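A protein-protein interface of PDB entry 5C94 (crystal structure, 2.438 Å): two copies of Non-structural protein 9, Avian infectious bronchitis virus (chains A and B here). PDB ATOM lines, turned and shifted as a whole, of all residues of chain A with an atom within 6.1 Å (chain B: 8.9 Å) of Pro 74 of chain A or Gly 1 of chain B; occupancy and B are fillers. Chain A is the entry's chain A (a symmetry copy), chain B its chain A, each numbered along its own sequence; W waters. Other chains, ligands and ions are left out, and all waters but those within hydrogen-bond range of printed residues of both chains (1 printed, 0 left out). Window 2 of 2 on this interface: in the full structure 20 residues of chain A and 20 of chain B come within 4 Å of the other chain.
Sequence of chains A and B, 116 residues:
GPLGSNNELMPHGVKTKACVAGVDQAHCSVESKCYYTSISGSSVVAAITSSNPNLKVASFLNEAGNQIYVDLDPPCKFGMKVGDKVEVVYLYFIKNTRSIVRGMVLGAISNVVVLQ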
ATOM      1  N   LEU A  72      11.922  24.590  29.208  1.00  0.00           N
ATOM      2  CA  LEU A  72      12.927  24.506  28.157  1.00  0.00           C
ATOM      3  C   LEU A  72      13.760  25.794  28.078  1.00  0.00           C
ATOM      4  O   LEU A  72      13.221  26.891  28.200  1.00  0.00           O
ATOM      5  CB  LEU A  72      12.243  24.236  26.809  1.00  0.00           C
ATOM      6  CG  LEU A  72      11.348  23.001  26.751  1.00  0.00           C
ATOM      7  CD1 LEU A  72      10.661  22.896  25.396  1.00  0.00           C
ATOM      8  CD2 LEU A  72      12.181  21.755  27.037  1.00  0.00           C
ATOM      9  N   ASP A  73      15.069  25.658  27.874  1.00  0.00           N
ATOM     10  CA  ASP A  73      15.894  26.793  27.474  1.00  0.00           C
ATOM     11  C   ASP A  73      15.486  27.247  26.068  1.00  0.00           C
ATOM     12  O   ASP A  73      14.762  26.539  25.363  1.00  0.00           O
ATOM     13  CB  ASP A  73      17.374  26.420  27.504  1.00  0.00           C
ATOM     14  CG  ASP A  73      17.910  26.229  28.918  1.00  0.00           C
ATOM     15  OD1 ASP A  73      17.279  26.704  29.887  1.00  0.00           O
ATOM     16  OD2 ASP A  73      18.988  25.613  29.056  1.00  0.00           O
ATOM     17  N   PRO A  74      15.933  28.435  25.642  1.00  0.00           N
ATOM     18  CA  PRO A  74      15.607  28.738  24.238  1.00  0.00           C
ATOM     19  C   PRO A  74      16.313  27.758  23.284  1.00  0.00           C
ATOM     20  O   PRO A  74      17.360  27.226  23.635  1.00  0.00           O
ATOM     21  CB  PRO A  74      16.124  30.163  24.056  1.00  0.00           C
ATOM     22  CG  PRO A  74      16.253  30.713  25.503  1.00  0.00           C
ATOM     23  CD  PRO A  74      16.640  29.542  26.318  1.00  0.00           C
ATOM     24  N   PRO A  75      15.749  27.527  22.090  1.00  0.00           N
ATOM     25  CA  PRO A  75      16.269  26.472  21.219  1.00  0.00           C
ATOM     26  C   PRO A  75      17.513  26.873  20.399  1.00  0.00           C
ATOM     27  O   PRO A  75      17.624  28.034  20.017  1.00  0.00           O
ATOM     28  CB  PRO A  75      15.083  26.202  20.288  1.00  0.00           C
ATOM     29  CG  PRO A  75      14.464  27.578  20.122  1.00  0.00           C
ATOM     30  CD  PRO A  75      14.554  28.184  21.513  1.00  0.00           C
ATOM     31  N   CYS A  76      18.421  25.915  20.168  1.00  0.00           N
ATOM     32  CA  CYS A  76      19.455  25.978  19.125  1.00  0.00           C
ATOM     33  C   CYS A  76      18.781  25.579  17.832  1.00  0.00           C
ATOM     34  O   CYS A  76      17.835  24.789  17.878  1.00  0.00           O
ATOM     35  CB  CYS A  76      20.565  24.951  19.335  1.00  0.00           C
ATOM     36  SG  CYS A  76      21.153  24.668  20.963  1.00  0.00           S
ATOM     37  N   LEU A  91      16.424  22.458  18.695  1.00  0.00           N
ATOM     38  CA  LEU A  91      16.863  21.607  19.789  1.00  0.00           C
ATOM     39  C   LEU A  91      16.805  22.416  21.082  1.00  0.00           C
ATOM     40  O   LEU A  91      17.446  23.474  21.201  1.00  0.00           O
ATOM     41  CB  LEU A  91      18.264  21.068  19.511  1.00  0.00           C
ATOM     42  CG  LEU A  91      19.018  20.100  20.441  1.00  0.00           C
ATOM     43  CD1 LEU A  91      19.774  20.870  21.468  1.00  0.00           C
ATOM     44  CD2 LEU A  91      18.130  19.097  21.116  1.00  0.00           C
ATOM     45  N   TYR A  92      15.994  21.930  22.020  1.00  0.00           N
ATOM     46  CA  TYR A  92      15.781  22.593  23.291  1.00  0.00           C
ATOM     47  C   TYR A  92      16.348  21.745  24.401  1.00  0.00           C
ATOM     48  O   TYR A  92      15.897  20.615  24.595  1.00  0.00           O
ATOM     49  CB  TYR A  92      14.292  22.799  23.599  1.00  0.00           C
ATOM     50  CG  TYR A  92      13.415  23.467  22.569  1.00  0.00           C
ATOM     51  CD1 TYR A  92      12.989  22.792  21.423  1.00  0.00           C
ATOM     52  CD2 TYR A  92      12.957  24.756  22.787  1.00  0.00           C
ATOM     53  CE1 TYR A  92      12.159  23.414  20.504  1.00  0.00           C
ATOM     54  CE2 TYR A  92      12.135  25.381  21.896  1.00  0.00           C
ATOM     55  CZ  TYR A  92      11.735  24.719  20.762  1.00  0.00           C
ATOM     56  OH  TYR A  92      10.900  25.386  19.910  1.00  0.00           O
ATOM     57  N   PHE A  93      17.299  22.275  25.148  1.00  0.00           N
ATOM     58  CA  PHE A  93      17.732  21.582  26.344  1.00  0.00           C
ATOM     59  C   PHE A  93      16.760  21.918  27.443  1.00  0.00           C
ATOM     60  O   PHE A  93      16.131  22.972  27.449  1.00  0.00           O
ATOM     61  CB  PHE A  93      19.153  21.960  26.750  1.00  0.00           C
ATOM     62  CG  PHE A  93      20.198  21.467  25.800  1.00  0.00           C
ATOM     63  CD1 PHE A  93      20.518  20.114  25.742  1.00  0.00           C
ATOM     64  CD2 PHE A  93      20.843  22.352  24.945  1.00  0.00           C
ATOM     65  CE1 PHE A  93      21.482  19.655  24.860  1.00  0.00           C
ATOM     66  CE2 PHE A  93      21.810  21.908  24.060  1.00  0.00           C
ATOM     67  CZ  PHE A  93      22.130  20.556  24.011  1.00  0.00           C
ATOM     68  N   LYS A  95      15.670  22.930  31.191  1.00  0.00           N
ATOM     69  CA  LYS A  95      16.174  23.881  32.171  1.00  0.00           C
ATOM     70  C   LYS A  95      17.074  23.177  33.170  1.00  0.00           C
ATOM     71  O   LYS A  95      16.670  22.158  33.750  1.00  0.00           O
ATOM     72  CB  LYS A  95      15.020  24.566  32.907  1.00  0.00           C
ATOM     73  CG  LYS A  95      15.106  26.082  32.973  1.00  0.00           C
ATOM     74  CD  LYS A  95      14.716  26.687  31.628  1.00  0.00           C
ATOM     75  CE  LYS A  95      14.490  28.193  31.700  1.00  0.00           C
ATOM     76  NZ  LYS A  95      14.256  28.781  30.342  1.00  0.00           N
ATOM     77  N   ARG A 102      24.334  18.015  28.369  1.00  0.00           N
ATOM     78  CA  ARG A 102      24.066  18.796  27.156  1.00  0.00           C
ATOM     79  C   ARG A 102      25.013  18.396  26.027  1.00  0.00           C
ATOM     80  O   ARG A 102      24.603  18.238  24.880  1.00  0.00           O
ATOM     81  CB  ARG A 102      24.207  20.298  27.415  1.00  0.00           C
ATOM     82  CG  ARG A 102      23.185  20.869  28.382  1.00  0.00           C
ATOM     83  CD  ARG A 102      23.398  22.359  28.624  1.00  0.00           C
ATOM     84  NE  ARG A 102      22.580  22.809  29.744  1.00  0.00           N
ATOM     85  CZ  ARG A 102      21.493  23.566  29.619  1.00  0.00           C
ATOM     86  NH1 ARG A 102      21.103  23.987  28.423  1.00  0.00           N
ATOM     87  NH2 ARG A 102      20.803  23.919  30.692  1.00  0.00           N
ATOM     88  N   GLY B   1      20.600  31.488  27.497  1.00  0.00           N
ATOM     89  CA  GLY B   1      20.570  31.029  26.120  1.00  0.00           C
ATOM     90  C   GLY B   1      20.447  29.521  26.059  1.00  0.00           C
ATOM     91  O   GLY B   1      20.299  28.881  27.100  1.00  0.00           O
ATOM     92  N   PRO B   2      20.507  28.950  24.842  1.00  0.00           N
ATOM     93  CA  PRO B   2      20.426  27.505  24.579  1.00  0.00           C
ATOM     94  C   PRO B   2      21.230  26.620  25.541  1.00  0.00           C
ATOM     95  O   PRO B   2      20.746  25.535  25.878  1.00  0.00           O
ATOM     96  CB  PRO B   2      20.981  27.393  23.161  1.00  0.00           C
ATOM     97  CG  PRO B   2      20.554  28.664  22.514  1.00  0.00           C
ATOM     98  CD  PRO B   2      20.605  29.724  23.590  1.00  0.00           C
ATOM     99  N   LEU B   3      22.412  27.061  25.976  1.00  0.00           N
ATOM    100  CA  LEU B   3      23.234  26.243  26.876  1.00  0.00           C
ATOM    101  C   LEU B   3      23.153  26.672  28.350  1.00  0.00           C
ATOM    102  O   LEU B   3      23.869  26.126  29.197  1.00  0.00           O
ATOM    103  CB  LEU B   3      24.701  26.237  26.421  1.00  0.00           C
ATOM    104  CG  LEU B   3      25.013  25.949  24.948  1.00  0.00           C
ATOM    105  CD1 LEU B   3      26.517  25.949  24.708  1.00  0.00           C
ATOM    106  CD2 LEU B   3      24.405  24.625  24.519  1.00  0.00           C
ATOM    107  N   GLY B   4      22.297  27.649  28.647  1.00  0.00           N
ATOM    108  CA  GLY B   4      21.890  27.917  30.017  1.00  0.00           C
ATOM    109  C   GLY B   4      22.592  29.006  30.812  1.00  0.00           C
ATOM    110  O   GLY B   4      22.809  30.111  30.315  1.00  0.00           O
ATOM    111  N   SER B   5      22.937  28.659  32.054  1.00  0.00           N
ATOM    112  CA  SER B   5      23.390  29.577  33.112  1.00  0.00           C
ATOM    113  C   SER B   5      24.449  30.681  33.146  1.00  0.00           C
ATOM    114  O   SER B   5      24.170  31.817  33.536  1.00  0.00           O
ATOM    115  CB  SER B   5      24.014  28.758  34.246  1.00  0.00           C
ATOM    116  OG  SER B   5      25.360  28.420  33.950  1.00  0.00           O
ATOM    117  N   ASN B   6      25.672  30.340  32.745  1.00  0.00           N
ATOM    118  CA  ASN B   6      26.714  31.342  32.555  1.00  0.00           C
ATOM    119  C   ASN B   6      27.000  31.010  31.092  1.00  0.00           C
ATOM    120  O   ASN B   6      28.122  31.181  30.613  1.00  0.00           O
ATOM    121  CB  ASN B   6      27.978  31.203  33.409  1.00  0.00           C
ATOM    122  N   ASN B   7      25.960  30.519  30.411  1.00  0.00           N
ATOM    123  CA  ASN B   7      25.969  30.228  28.984  1.00  0.00           C
ATOM    124  C   ASN B   7      27.221  29.309  28.691  1.00  0.00           C
ATOM    125  O   ASN B   7      27.406  28.378  29.483  1.00  0.00           O
ATOM    126  CB  ASN B   7      25.848  31.568  28.237  1.00  0.00           C
ATOM    127  N   GLU B   8      28.066  29.447  27.654  1.00  0.00           N
ATOM    128  CA  GLU B   8      28.016  30.371  26.527  1.00  0.00           C
ATOM    129  C   GLU B   8      28.379  29.796  25.178  1.00  0.00           C
ATOM    130  O   GLU B   8      27.557  29.767  24.262  1.00  0.00           O
ATOM    131  CB  GLU B   8      28.949  31.567  26.764  1.00  0.00           C
HETATM  132  O   HOH W   1      18.386  24.728  24.410  1.00  0.00           O
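Among the printed residues, pairs that only touch across the chains: Pro 74 of chain A with Pro 2 of chain B (3.2 Å), Phe 93 of chain A with Pro 2 of chain B (3.3 Å), Arg 102 of chain A with Leu 3 of chain B (3.4 Å), Cys 76 of chain A with Pro 2 of chain B (3.5 Å), Asp 73 of chain A with Pro 2 of chain B (3.6 Å), Phe 93 of chain A with Leu 3 of chain B (3.8 Å), Pro 74 of chain A with Gly 1 of chain B (3.8 Å), Asp 73 of chain A with Gly 4 of chain B (3.8 Å), Asp 73 of chain A with Gly 1 of chain B (3.8 Å), Arg 102 of chain A with Gly 4 of chain B (3.9 Å) and Pro 75 of chain A with Pro 2 of chain B (3.9 Å).
No position is printed for both chains.
Of the 12 pairs that touch across the chains among the printed residues, none has its exchanged pair printed and touching as well.
NH1 of Arg 102 of chain A lies within hydrogen-bond range of O of Pro 2 of chain B (3.0 Å).
Water W1 lies within hydrogen-bond range of N of Phe 93 of chain A, O of Pro 74 of chain A and O of Pro 2 of chain B.
The backbone NH of Asp 73 of chain A lies within hydrogen-bond range of the backbone carbonyl oxygen of Phe 93 of chain A, at 2.9 Å.
The side-chain amino group of Lys 95 of chain A is in salt-bridge range of the side-chain carboxylate of Asp 73 of chain A.
The guanidinium group (NH1) of Arg 102 of chain A lies within salt-bridge range of the side-chain carboxylate (OD2) of Asp 73 of chain A, 2.7 Å away.
The backbone NH of Cys 76 of chain A lies within hydrogen-bond range of the backbone carbonyl oxygen of Leu 91 of chain A (2.8 Å).
Of chain B, only Gly 1 and Pro 2 come within 4 Å of Pro 74 of chain A.
Gly 1 of chain B touches just these residues of chain A: Asp 73 (3.8 Å) and Pro 74 (3.8 Å).
Of chain B, only Gly 1, Pro 2 and Gly 4 come within 4 Å of Asp 73 of chain A.
Of chain B, only Pro 2 comes within 4 Å of Pro 75 of chain A.
Of the printed residues of chain A, Leu 3 of chain B touches Phe 93 (3.8 Å) and Arg 102 (3.4 Å).
Printed residues of chain B within 4 Å of Phe 93 of chain A: Pro 2 (3.3 Å) and Leu 3 (3.8 Å).
Printed residues of chain B within 4 Å of Cys 76 of chain A: Pro 2 (3.5 Å).
Ser 5 of chain B touches none of the printed residues of chain A.
Tyr 92 of chain A touches none of the printed residues of chain B.
The nearest residue of chain B that does not touch Pro 74 of chain A is Leu 3 of chain B (5.6 Å).
The nearest printed residue of chain A that does not touch Gly 4 of chain B is Pro 74 of chain A (6.4 Å).
Printed residues of chain A that touch a printed residue of chain B: Asp 73, Pro 74, Pro 75, Cys 76, Phe 93 and Arg 102.
Along chain B the printed residues that touch a printed residue of chain A span positions 1 to 4.
Among the printed residues, 12 pairs touch across the chains.
Among the printed residues, no Asp or Glu carboxylate lies within 4 Å of a Lys or Arg side-chain nitrogen of the other chain.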
